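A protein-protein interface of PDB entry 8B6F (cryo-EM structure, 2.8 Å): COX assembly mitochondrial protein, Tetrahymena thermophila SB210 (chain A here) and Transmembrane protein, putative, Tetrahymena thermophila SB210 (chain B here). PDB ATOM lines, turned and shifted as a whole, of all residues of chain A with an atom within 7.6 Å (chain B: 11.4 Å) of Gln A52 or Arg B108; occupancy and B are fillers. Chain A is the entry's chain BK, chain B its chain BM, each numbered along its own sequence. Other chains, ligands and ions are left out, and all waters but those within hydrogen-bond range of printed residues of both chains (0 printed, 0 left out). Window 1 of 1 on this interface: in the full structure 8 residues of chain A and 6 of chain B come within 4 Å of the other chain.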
ATOM      1  N   LYS A  47      -1.047  -6.428 -35.445  1.00  0.00           N
ATOM      2  CA  LYS A  47      -0.118  -5.570 -34.727  1.00  0.00           C
ATOM      3  C   LYS A  47      -0.845  -4.905 -33.570  1.00  0.00           C
ATOM      4  O   LYS A  47      -2.077  -4.867 -33.526  1.00  0.00           O
ATOM      5  CB  LYS A  47       0.493  -4.516 -35.656  1.00  0.00           C
ATOM      6  CG  LYS A  47      -0.547  -3.714 -36.428  1.00  0.00           C
ATOM      7  CD  LYS A  47       0.089  -2.822 -37.482  1.00  0.00           C
ATOM      8  CE  LYS A  47       0.858  -1.672 -36.865  1.00  0.00           C
ATOM      9  NZ  LYS A  47      -0.022  -0.766 -36.078  1.00  0.00           N
ATOM     10  N   LEU A  48      -0.062  -4.382 -32.632  1.00  0.00           N
ATOM     11  CA  LEU A  48      -0.613  -3.595 -31.546  1.00  0.00           C
ATOM     12  C   LEU A  48      -1.081  -2.243 -32.075  1.00  0.00           C
ATOM     13  O   LEU A  48      -0.646  -1.799 -33.140  1.00  0.00           O
ATOM     14  CB  LEU A  48       0.425  -3.398 -30.445  1.00  0.00           C
ATOM     15  CG  LEU A  48       0.797  -4.632 -29.618  1.00  0.00           C
ATOM     16  CD1 LEU A  48       1.824  -5.488 -30.342  1.00  0.00           C
ATOM     17  CD2 LEU A  48       1.313  -4.222 -28.251  1.00  0.00           C
ATOM     18  N   PRO A  49      -1.979  -1.568 -31.352  1.00  0.00           N
ATOM     19  CA  PRO A  49      -2.496  -0.287 -31.867  1.00  0.00           C
ATOM     20  C   PRO A  49      -1.409   0.734 -32.158  1.00  0.00           C
ATOM     21  O   PRO A  49      -1.511   1.466 -33.150  1.00  0.00           O
ATOM     22  CB  PRO A  49      -3.440   0.183 -30.748  1.00  0.00           C
ATOM     23  CG  PRO A  49      -3.058  -0.612 -29.542  1.00  0.00           C
ATOM     24  CD  PRO A  49      -2.588  -1.927 -30.061  1.00  0.00           C
ATOM     25  N   GLY A  50      -0.373   0.806 -31.329  1.00  0.00           N
ATOM     26  CA  GLY A  50       0.697   1.763 -31.503  1.00  0.00           C
ATOM     27  C   GLY A  50       1.975   1.209 -32.096  1.00  0.00           C
ATOM     28  O   GLY A  50       2.971   1.939 -32.161  1.00  0.00           O
ATOM     29  N   GLN A  51       1.988  -0.046 -32.530  1.00  0.00           N
ATOM     30  CA  GLN A  51       3.198  -0.649 -33.067  1.00  0.00           C
ATOM     31  C   GLN A  51       3.452  -0.176 -34.492  1.00  0.00           C
ATOM     32  O   GLN A  51       2.519   0.005 -35.280  1.00  0.00           O
ATOM     33  CB  GLN A  51       3.089  -2.173 -33.031  1.00  0.00           C
ATOM     34  CG  GLN A  51       4.335  -2.894 -33.509  1.00  0.00           C
ATOM     35  CD  GLN A  51       4.245  -4.392 -33.313  1.00  0.00           C
ATOM     36  OE1 GLN A  51       3.179  -4.928 -33.020  1.00  0.00           O
ATOM     37  NE2 GLN A  51       5.371  -5.076 -33.472  1.00  0.00           N
ATOM     38  N   GLN A  52       4.726   0.023 -34.820  1.00  0.00           N
ATOM     39  CA  GLN A  52       5.142   0.396 -36.163  1.00  0.00           C
ATOM     40  C   GLN A  52       6.476  -0.274 -36.457  1.00  0.00           C
ATOM     41  O   GLN A  52       7.211  -0.659 -35.546  1.00  0.00           O
ATOM     42  CB  GLN A  52       5.266   1.917 -36.324  1.00  0.00           C
ATOM     43  CG  GLN A  52       3.978   2.684 -36.065  1.00  0.00           C
ATOM     44  CD  GLN A  52       2.899   2.381 -37.085  1.00  0.00           C
ATOM     45  OE1 GLN A  52       3.162   1.777 -38.122  1.00  0.00           O
ATOM     46  NE2 GLN A  52       1.675   2.804 -36.794  1.00  0.00           N
ATOM     47  N   TYR A  53       6.784  -0.410 -37.744  1.00  0.00           N
ATOM     48  CA  TYR A  53       7.980  -1.108 -38.194  1.00  0.00           C
ATOM     49  C   TYR A  53       8.915  -0.131 -38.888  1.00  0.00           C
ATOM     50  O   TYR A  53       8.490   0.613 -39.778  1.00  0.00           O
ATOM     51  CB  TYR A  53       7.620  -2.253 -39.146  1.00  0.00           C
ATOM     52  CG  TYR A  53       6.608  -3.219 -38.578  1.00  0.00           C
ATOM     53  CD1 TYR A  53       6.973  -4.158 -37.624  1.00  0.00           C
ATOM     54  CD2 TYR A  53       5.286  -3.192 -38.999  1.00  0.00           C
ATOM     55  CE1 TYR A  53       6.051  -5.042 -37.103  1.00  0.00           C
ATOM     56  CE2 TYR A  53       4.355  -4.072 -38.483  1.00  0.00           C
ATOM     57  CZ  TYR A  53       4.745  -4.995 -37.536  1.00  0.00           C
ATOM     58  OH  TYR A  53       3.824  -5.874 -37.020  1.00  0.00           O
ATOM     59  N   ASP A  54      10.185  -0.135 -38.481  1.00  0.00           N
ATOM     60  CA  ASP A  54      11.217   0.664 -39.139  1.00  0.00           C
ATOM     61  C   ASP A  54      11.856  -0.215 -40.205  1.00  0.00           C
ATOM     62  O   ASP A  54      12.846  -0.905 -39.967  1.00  0.00           O
ATOM     63  CB  ASP A  54      12.240   1.169 -38.131  1.00  0.00           C
ATOM     64  CG  ASP A  54      13.191   2.184 -38.729  1.00  0.00           C
ATOM     65  OD1 ASP A  54      13.028   2.525 -39.918  1.00  0.00           O
ATOM     66  OD2 ASP A  54      14.104   2.640 -38.009  1.00  0.00           O
ATOM     67  N   TYR A  55      11.273  -0.185 -41.403  1.00  0.00           N
ATOM     68  CA  TYR A  55      11.677  -1.114 -42.451  1.00  0.00           C
ATOM     69  C   TYR A  55      13.118  -0.879 -42.885  1.00  0.00           C
ATOM     70  O   TYR A  55      13.852  -1.835 -43.154  1.00  0.00           O
ATOM     71  CB  TYR A  55      10.730  -0.994 -43.642  1.00  0.00           C
ATOM     72  CG  TYR A  55       9.370  -1.603 -43.390  1.00  0.00           C
ATOM     73  CD1 TYR A  55       9.199  -2.980 -43.362  1.00  0.00           C
ATOM     74  CD2 TYR A  55       8.257  -0.800 -43.184  1.00  0.00           C
ATOM     75  CE1 TYR A  55       7.956  -3.540 -43.134  1.00  0.00           C
ATOM     76  CE2 TYR A  55       7.013  -1.348 -42.954  1.00  0.00           C
ATOM     77  CZ  TYR A  55       6.867  -2.718 -42.930  1.00  0.00           C
ATOM     78  OH  TYR A  55       5.627  -3.265 -42.702  1.00  0.00           O
ATOM     79  N   ARG A  57      15.739   0.176 -41.130  1.00  0.00           N
ATOM     80  CA  ARG A  57      16.659  -0.427 -40.173  1.00  0.00           C
ATOM     81  C   ARG A  57      16.556  -1.947 -40.192  1.00  0.00           C
ATOM     82  O   ARG A  57      17.576  -2.643 -40.180  1.00  0.00           O
ATOM     83  CB  ARG A  57      16.381   0.122 -38.776  1.00  0.00           C
ATOM     84  CG  ARG A  57      17.380  -0.323 -37.724  1.00  0.00           C
ATOM     85  CD  ARG A  57      17.302   0.560 -36.490  1.00  0.00           C
ATOM     86  NE  ARG A  57      15.999   0.484 -35.839  1.00  0.00           N
ATOM     87  CZ  ARG A  57      15.698  -0.323 -34.830  1.00  0.00           C
ATOM     88  NH1 ARG A  57      16.589  -1.155 -34.317  1.00  0.00           N
ATOM     89  NH2 ARG A  57      14.470  -0.290 -34.318  1.00  0.00           N
ATOM     90  N   SER A  92      16.446  -5.355 -34.560  1.00  0.00           N
ATOM     91  CA  SER A  92      15.891  -4.452 -35.561  1.00  0.00           C
ATOM     92  C   SER A  92      14.579  -4.961 -36.141  1.00  0.00           C
ATOM     93  O   SER A  92      13.645  -4.177 -36.336  1.00  0.00           O
ATOM     94  CB  SER A  92      16.907  -4.235 -36.681  1.00  0.00           C
ATOM     95  OG  SER A  92      18.101  -3.664 -36.177  1.00  0.00           O
ATOM     96  N   ASP A  94      11.073  -7.413 -36.583  1.00  0.00           N
ATOM     97  CA  ASP A  94       9.994  -7.980 -35.793  1.00  0.00           C
ATOM     98  C   ASP A  94       9.905  -9.488 -36.011  1.00  0.00           C
ATOM     99  O   ASP A  94      10.450 -10.041 -36.969  1.00  0.00           O
ATOM    100  CB  ASP A  94       8.667  -7.311 -36.158  1.00  0.00           C
ATOM    101  CG  ASP A  94       7.550  -7.666 -35.198  1.00  0.00           C
ATOM    102  OD1 ASP A  94       7.622  -7.260 -34.021  1.00  0.00           O
ATOM    103  OD2 ASP A  94       6.596  -8.349 -35.625  1.00  0.00           O
ATOM    104  N   GLY B 100      -1.136   7.988 -20.419  1.00  0.00           N
ATOM    105  CA  GLY B 100      -1.957   6.917 -20.957  1.00  0.00           C
ATOM    106  C   GLY B 100      -1.994   6.932 -22.473  1.00  0.00           C
ATOM    107  O   GLY B 100      -1.892   5.887 -23.117  1.00  0.00           O
ATOM    108  N   HIS B 101      -2.138   8.120 -23.062  1.00  0.00           N
ATOM    109  CA  HIS B 101      -2.083   8.240 -24.514  1.00  0.00           C
ATOM    110  C   HIS B 101      -0.714   7.833 -25.043  1.00  0.00           C
ATOM    111  O   HIS B 101      -0.604   6.983 -25.931  1.00  0.00           O
ATOM    112  CB  HIS B 101      -2.400   9.676 -24.934  1.00  0.00           C
ATOM    113  CG  HIS B 101      -3.808  10.102 -24.654  1.00  0.00           C
ATOM    114  ND1 HIS B 101      -4.595  10.732 -25.594  1.00  0.00           N
ATOM    115  CD2 HIS B 101      -4.569   9.994 -23.539  1.00  0.00           C
ATOM    116  CE1 HIS B 101      -5.779  10.993 -25.071  1.00  0.00           C
ATOM    117  NE2 HIS B 101      -5.790  10.556 -23.825  1.00  0.00           N
ATOM    118  N   THR B 102       0.347   8.423 -24.493  1.00  0.00           N
ATOM    119  CA  THR B 102       1.663   8.283 -25.108  1.00  0.00           C
ATOM    120  C   THR B 102       2.165   6.845 -25.036  1.00  0.00           C
ATOM    121  O   THR B 102       2.788   6.356 -25.984  1.00  0.00           O
ATOM    122  CB  THR B 102       2.658   9.246 -24.452  1.00  0.00           C
ATOM    123  OG1 THR B 102       3.814   9.382 -25.287  1.00  0.00           O
ATOM    124  CG2 THR B 102       3.111   8.738 -23.097  1.00  0.00           C
ATOM    125  N   PHE B 103       1.919   6.154 -23.921  1.00  0.00           N
ATOM    126  CA  PHE B 103       2.399   4.781 -23.802  1.00  0.00           C
ATOM    127  C   PHE B 103       1.793   3.887 -24.873  1.00  0.00           C
ATOM    128  O   PHE B 103       2.509   3.164 -25.575  1.00  0.00           O
ATOM    129  CB  PHE B 103       2.082   4.217 -22.417  1.00  0.00           C
ATOM    130  CG  PHE B 103       2.415   2.762 -22.282  1.00  0.00           C
ATOM    131  CD1 PHE B 103       3.710   2.358 -22.013  1.00  0.00           C
ATOM    132  CD2 PHE B 103       1.438   1.797 -22.449  1.00  0.00           C
ATOM    133  CE1 PHE B 103       4.025   1.022 -21.901  1.00  0.00           C
ATOM    134  CE2 PHE B 103       1.745   0.456 -22.339  1.00  0.00           C
ATOM    135  CZ  PHE B 103       3.040   0.069 -22.064  1.00  0.00           C
ATOM    136  N   VAL B 104       0.469   3.923 -25.017  1.00  0.00           N
ATOM    137  CA  VAL B 104      -0.187   3.073 -26.003  1.00  0.00           C
ATOM    138  C   VAL B 104       0.208   3.489 -27.412  1.00  0.00           C
ATOM    139  O   VAL B 104       0.348   2.647 -28.306  1.00  0.00           O
ATOM    140  CB  VAL B 104      -1.713   3.112 -25.807  1.00  0.00           C
ATOM    141  CG1 VAL B 104      -2.415   2.267 -26.862  1.00  0.00           C
ATOM    142  CG2 VAL B 104      -2.080   2.633 -24.412  1.00  0.00           C
ATOM    143  N   GLN B 105       0.399   4.789 -27.633  1.00  0.00           N
ATOM    144  CA  GLN B 105       0.734   5.264 -28.969  1.00  0.00           C
ATOM    145  C   GLN B 105       2.136   4.845 -29.388  1.00  0.00           C
ATOM    146  O   GLN B 105       2.371   4.589 -30.574  1.00  0.00           O
ATOM    147  CB  GLN B 105       0.590   6.783 -29.021  1.00  0.00           C
ATOM    148  CG  GLN B 105      -0.838   7.274 -28.845  1.00  0.00           C
ATOM    149  CD  GLN B 105      -1.684   7.052 -30.072  1.00  0.00           C
ATOM    150  OE1 GLN B 105      -1.271   6.371 -31.010  1.00  0.00           O
ATOM    151  NE2 GLN B 105      -2.871   7.649 -30.087  1.00  0.00           N
ATOM    152  N   ASN B 106       3.077   4.770 -28.446  1.00  0.00           N
ATOM    153  CA  ASN B 106       4.482   4.544 -28.765  1.00  0.00           C
ATOM    154  C   ASN B 106       5.043   3.312 -28.063  1.00  0.00           C
ATOM    155  O   ASN B 106       6.246   3.236 -27.815  1.00  0.00           O
ATOM    156  CB  ASN B 106       5.313   5.773 -28.394  1.00  0.00           C
ATOM    157  CG  ASN B 106       4.772   7.047 -29.000  1.00  0.00           C
ATOM    158  OD1 ASN B 106       4.328   7.064 -30.144  1.00  0.00           O
ATOM    159  ND2 ASN B 106       4.805   8.126 -28.230  1.00  0.00           N
ATOM    160  N   TYR B 107       4.195   2.334 -27.738  1.00  0.00           N
ATOM    161  CA  TYR B 107       4.679   1.161 -27.013  1.00  0.00           C
ATOM    162  C   TYR B 107       5.719   0.401 -27.827  1.00  0.00           C
ATOM    163  O   TYR B 107       6.891   0.314 -27.442  1.00  0.00           O
ATOM    164  CB  TYR B 107       3.505   0.249 -26.650  1.00  0.00           C
ATOM    165  CG  TYR B 107       3.873  -0.922 -25.758  1.00  0.00           C
ATOM    166  CD1 TYR B 107       5.080  -0.954 -25.067  1.00  0.00           C
ATOM    167  CD2 TYR B 107       3.011  -2.001 -25.618  1.00  0.00           C
ATOM    168  CE1 TYR B 107       5.413  -2.023 -24.260  1.00  0.00           C
ATOM    169  CE2 TYR B 107       3.337  -3.075 -24.811  1.00  0.00           C
ATOM    170  CZ  TYR B 107       4.540  -3.080 -24.135  1.00  0.00           C
ATOM    171  OH  TYR B 107       4.868  -4.145 -23.332  1.00  0.00           O
ATOM    172  N   ARG B 108       5.305  -0.156 -28.964  1.00  0.00           N
ATOM    173  CA  ARG B 108       6.194  -0.874 -29.869  1.00  0.00           C
ATOM    174  C   ARG B 108       6.384  -0.110 -31.174  1.00  0.00           C
ATOM    175  O   ARG B 108       6.512  -0.710 -32.243  1.00  0.00           O
ATOM    176  CB  ARG B 108       5.656  -2.276 -30.148  1.00  0.00           C
ATOM    177  CG  ARG B 108       5.517  -3.151 -28.914  1.00  0.00           C
ATOM    178  CD  ARG B 108       6.854  -3.354 -28.222  1.00  0.00           C
ATOM    179  NE  ARG B 108       6.778  -4.366 -27.177  1.00  0.00           N
ATOM    180  CZ  ARG B 108       7.786  -4.699 -26.382  1.00  0.00           C
ATOM    181  NH1 ARG B 108       8.966  -4.109 -26.477  1.00  0.00           N
ATOM    182  NH2 ARG B 108       7.605  -5.650 -25.470  1.00  0.00           N
ATOM    183  N   ASN B 109       6.401   1.217 -31.095  1.00  0.00           N
ATOM    184  CA  ASN B 109       6.467   2.073 -32.275  1.00  0.00           C
ATOM    185  C   ASN B 109       7.933   2.293 -32.620  1.00  0.00           C
ATOM    186  O   ASN B 109       8.611   3.120 -32.006  1.00  0.00           O
ATOM    187  CB  ASN B 109       5.746   3.390 -32.010  1.00  0.00           C
ATOM    188  CG  ASN B 109       5.467   4.164 -33.273  1.00  0.00           C
ATOM    189  OD1 ASN B 109       6.216   4.079 -34.242  1.00  0.00           O
ATOM    190  ND2 ASN B 109       4.382   4.931 -33.271  1.00  0.00           N
ATOM    191  N   GLN B 110       8.428   1.549 -33.611  1.00  0.00           N
ATOM    192  CA  GLN B 110       9.812   1.710 -34.036  1.00  0.00           C
ATOM    193  C   GLN B 110      10.050   3.048 -34.722  1.00  0.00           C
ATOM    194  O   GLN B 110      11.198   3.496 -34.794  1.00  0.00           O
ATOM    195  CB  GLN B 110      10.213   0.569 -34.970  1.00  0.00           C
ATOM    196  CG  GLN B 110      10.210  -0.798 -34.305  1.00  0.00           C
ATOM    197  CD  GLN B 110      10.747  -1.886 -35.212  1.00  0.00           C
ATOM    198  OE1 GLN B 110      11.172  -1.620 -36.334  1.00  0.00           O
ATOM    199  NE2 GLN B 110      10.730  -3.122 -34.727  1.00  0.00           N
ATOM    200  N   ALA B 111       8.996   3.691 -35.232  1.00  0.00           N
ATOM    201  CA  ALA B 111       9.166   4.999 -35.854  1.00  0.00           C
ATOM    202  C   ALA B 111       9.652   6.027 -34.841  1.00  0.00           C
ATOM    203  O   ALA B 111      10.519   6.853 -35.150  1.00  0.00           O
ATOM    204  CB  ALA B 111       7.853   5.453 -36.493  1.00  0.00           C
ATOM    205  N   THR B 112       9.104   5.996 -33.626  1.00  0.00           N
ATOM    206  CA  THR B 112       9.542   6.888 -32.562  1.00  0.00           C
ATOM    207  C   THR B 112      10.659   6.274 -31.727  1.00  0.00           C
ATOM    208  O   THR B 112      11.632   6.960 -31.400  1.00  0.00           O
ATOM    209  CB  THR B 112       8.362   7.253 -31.658  1.00  0.00           C
ATOM    210  OG1 THR B 112       7.774   6.059 -31.128  1.00  0.00           O
ATOM    211  CG2 THR B 112       7.310   8.031 -32.437  1.00  0.00           C
ATOM    212  N   ASP B 113      10.537   4.994 -31.379  1.00  0.00           N
ATOM    213  CA  ASP B 113      11.565   4.265 -30.640  1.00  0.00           C
ATOM    214  C   ASP B 113      11.996   5.039 -29.394  1.00  0.00           C
ATOM    215  O   ASP B 113      13.143   5.463 -29.251  1.00  0.00           O
ATOM    216  CB  ASP B 113      12.763   3.968 -31.544  1.00  0.00           C
ATOM    217  CG  ASP B 113      13.839   3.165 -30.838  1.00  0.00           C
ATOM    218  OD1 ASP B 113      13.593   1.981 -30.527  1.00  0.00           O
ATOM    219  OD2 ASP B 113      14.931   3.720 -30.593  1.00  0.00           O
ATOM    220  N   LEU B 114      11.038   5.222 -28.486  1.00  0.00           N
ATOM    221  CA  LEU B 114      11.300   6.000 -27.280  1.00  0.00           C
ATOM    222  C   LEU B 114      12.112   5.214 -26.256  1.00  0.00           C
ATOM    223  O   LEU B 114      12.938   5.795 -25.546  1.00  0.00           O
ATOM    224  CB  LEU B 114       9.978   6.472 -26.675  1.00  0.00           C
ATOM    225  CG  LEU B 114       9.152   7.401 -27.572  1.00  0.00           C
ATOM    226  CD1 LEU B 114       7.830   7.748 -26.920  1.00  0.00           C
ATOM    227  CD2 LEU B 114       9.920   8.670 -27.908  1.00  0.00           C
ATOM    228  N   GLY B 115      11.895   3.906 -26.160  1.00  0.00           N
ATOM    229  CA  GLY B 115      12.668   3.077 -25.255  1.00  0.00           C
ATOM    230  C   GLY B 115      11.847   2.488 -24.128  1.00  0.00           C
ATOM    231  O   GLY B 115      10.636   2.298 -24.268  1.00  0.00           O
ATOM    232  N   ARG B 116      12.494   2.194 -23.002  1.00  0.00           N
ATOM    233  CA  ARG B 116      11.796   1.611 -21.867  1.00  0.00           C
ATOM    234  C   ARG B 116      10.914   2.653 -21.190  1.00  0.00           C
ATOM    235  O   ARG B 116      11.073   3.862 -21.379  1.00  0.00           O
ATOM    236  CB  ARG B 116      12.790   1.032 -20.861  1.00  0.00           C
ATOM    237  CG  ARG B 116      13.598  -0.139 -21.396  1.00  0.00           C
ATOM    238  CD  ARG B 116      14.489  -0.728 -20.317  1.00  0.00           C
ATOM    239  NE  ARG B 116      15.414   0.263 -19.782  1.00  0.00           N
ATOM    240  CZ  ARG B 116      16.212   0.063 -18.743  1.00  0.00           C
ATOM    241  NH1 ARG B 116      16.221  -1.086 -18.088  1.00  0.00           N
ATOM    242  NH2 ARG B 116      17.022   1.041 -18.349  1.00  0.00           N
ATOM    243  N   TRP B 117       9.975   2.170 -20.384  1.00  0.00           N
ATOM    244  CA  TRP B 117       8.974   3.009 -19.739  1.00  0.00           C
ATOM    245  C   TRP B 117       9.299   3.145 -18.259  1.00  0.00           C
ATOM    246  O   TRP B 117       9.539   2.145 -17.575  1.00  0.00           O
ATOM    247  CB  TRP B 117       7.572   2.419 -19.919  1.00  0.00           C
ATOM    248  CG  TRP B 117       6.480   3.219 -19.271  1.00  0.00           C
ATOM    249  CD1 TRP B 117       5.957   3.031 -18.026  1.00  0.00           C
ATOM    250  CD2 TRP B 117       5.773   4.327 -19.840  1.00  0.00           C
ATOM    251  NE1 TRP B 117       4.970   3.954 -17.783  1.00  0.00           N
ATOM    252  CE2 TRP B 117       4.838   4.762 -18.882  1.00  0.00           C
ATOM    253  CE3 TRP B 117       5.843   4.995 -21.066  1.00  0.00           C
ATOM    254  CZ2 TRP B 117       3.979   5.834 -19.111  1.00  0.00           C
ATOM    255  CZ3 TRP B 117       4.987   6.059 -21.293  1.00  0.00           C
ATOM    256  CH2 TRP B 117       4.068   6.468 -20.320  1.00  0.00           C
ATOM    257  N   TYR B 124       8.770   7.631 -21.053  1.00  0.00           N
ATOM    258  CA  TYR B 124       9.828   6.842 -21.656  1.00  0.00           C
ATOM    259  C   TYR B 124      11.193   7.439 -21.332  1.00  0.00           C
ATOM    260  O   TYR B 124      11.315   8.597 -20.926  1.00  0.00           O
ATOM    261  CB  TYR B 124       9.647   6.759 -23.171  1.00  0.00           C
ATOM    262  CG  TYR B 124       8.496   5.887 -23.615  1.00  0.00           C
ATOM    263  CD1 TYR B 124       8.629   4.506 -23.667  1.00  0.00           C
ATOM    264  CD2 TYR B 124       7.283   6.443 -23.994  1.00  0.00           C
ATOM    265  CE1 TYR B 124       7.587   3.705 -24.079  1.00  0.00           C
ATOM    266  CE2 TYR B 124       6.234   5.648 -24.407  1.00  0.00           C
ATOM    267  CZ  TYR B 124       6.393   4.280 -24.449  1.00  0.00           C
ATOM    268  OH  TYR B 124       5.356   3.477 -24.859  1.00  0.00           O
ATOM    269  N   GLU B 125      12.231   6.625 -21.522  1.00  0.00           N
ATOM    270  CA  GLU B 125      13.584   7.077 -21.221  1.00  0.00           C
ATOM    271  C   GLU B 125      13.977   8.270 -22.080  1.00  0.00           C
ATOM    272  O   GLU B 125      14.579   9.231 -21.585  1.00  0.00           O
ATOM    273  CB  GLU B 125      14.578   5.933 -21.421  1.00  0.00           C
ATOM    274  CG  GLU B 125      14.497   4.846 -20.366  1.00  0.00           C
ATOM    275  CD  GLU B 125      15.498   3.732 -20.609  1.00  0.00           C
ATOM    276  OE1 GLU B 125      15.892   3.528 -21.775  1.00  0.00           O
ATOM    277  OE2 GLU B 125      15.896   3.064 -19.631  1.00  0.00           O
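N of Asp A54 is in hydrogen-bond range of OE1 of Gln B110 (2.8 Å). O of Gly A50 lies close to ND2 of Asn B109 (3.5 Å). The backbone carbonyl oxygen of Arg B108 is in hydrogen-bond range of the backbone NH of Gln A52 (3.2 Å). The backbone carbonyl oxygen of Ser A92 sits at hydrogen-bond distance from the side-chain amide nitrogen of Gln B110 (3.5 Å). The backbone carbonyl oxygen (O) of Gly A50 lies close to the backbone carbonyl oxygen (O) of Gln B105, 3.1 Å away. O of Gln A52 sits at hydrogen-bond distance from N of Gln B110 (3.2 Å).
Gln A52 touches just these residues of chain B: Arg B108 (3.2 Å), Asn B109 (3.1 Å) and Gln B110 (3.2 Å). Arg B108 touches two residues of chain A. Leu A48 touches one residue of chain B. Gly A50 touches just these residues of chain B: Val B104, Gln B105 and Asn B109. Gln A51 touches just one residue of chain B: Arg B108 (3.3 Å). Tyr A53 touches one residue of chain B. Printed residues of chain A within 4 Å of Tyr B107: Leu A48. Of the printed residues of chain A, Asn B109 touches Gly A50 and Gln A52. Printed residues of chain B within 4 Å of Asp A54: Gln B110 (2.8 Å). The nearest residue of chain A that does not touch Arg B108 is Gly A50 (4.1 Å).
Of the 20 printed residues of chain B, 6 touch a printed residue of chain A. Hydrophobic or aromatic side chains of chain A that line the printed part of chain B: Leu A48 and Pro A49. Among the printed residues, 12 pairs touch across the chains. Among the printed residues, no Asp or Glu carboxylate lies within 4 Å of a Lys or Arg side-chain nitrogen of the other chain.
The side-chain carboxylate of Asp A54 is in salt-bridge range of the guanidinium group of Arg A57 (3.6 Å). The side-chain amino group (NZ) of Lys A47 is in hydrogen-bond range of the backbone carbonyl oxygen (O) of Gln A51, 2.8 Å away. The backbone carbonyl oxygen (O) of Gln B105 sits at hydrogen-bond distance from the side-chain amide nitrogen (ND2) of Asn B109 (3.4 Å). The guanidinium group (NH1) of Arg A57 lies within hydrogen-bond range of the side-chain hydroxyl (OG) of Ser A92 (3.5 Å). The backbone NH of Tyr B107 lies close to the side-chain hydroxyl of Tyr B124 (3.3 Å). OD1 of Asn B109 is in hydrogen-bond range of N of Ala B111.
Among the printed residues, pairs that only touch across the chains: Gln A52 with Asn B109 (3.1 Å), Gln A51 with Arg B108 (3.3 Å), Gly A50 with Val B104 (3.3 Å), Tyr A53 with Gln B110 (3.7 Å), Leu A48 with Tyr B107 (3.8 Å) and Pro A49 with Val B104 (3.99 Å).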
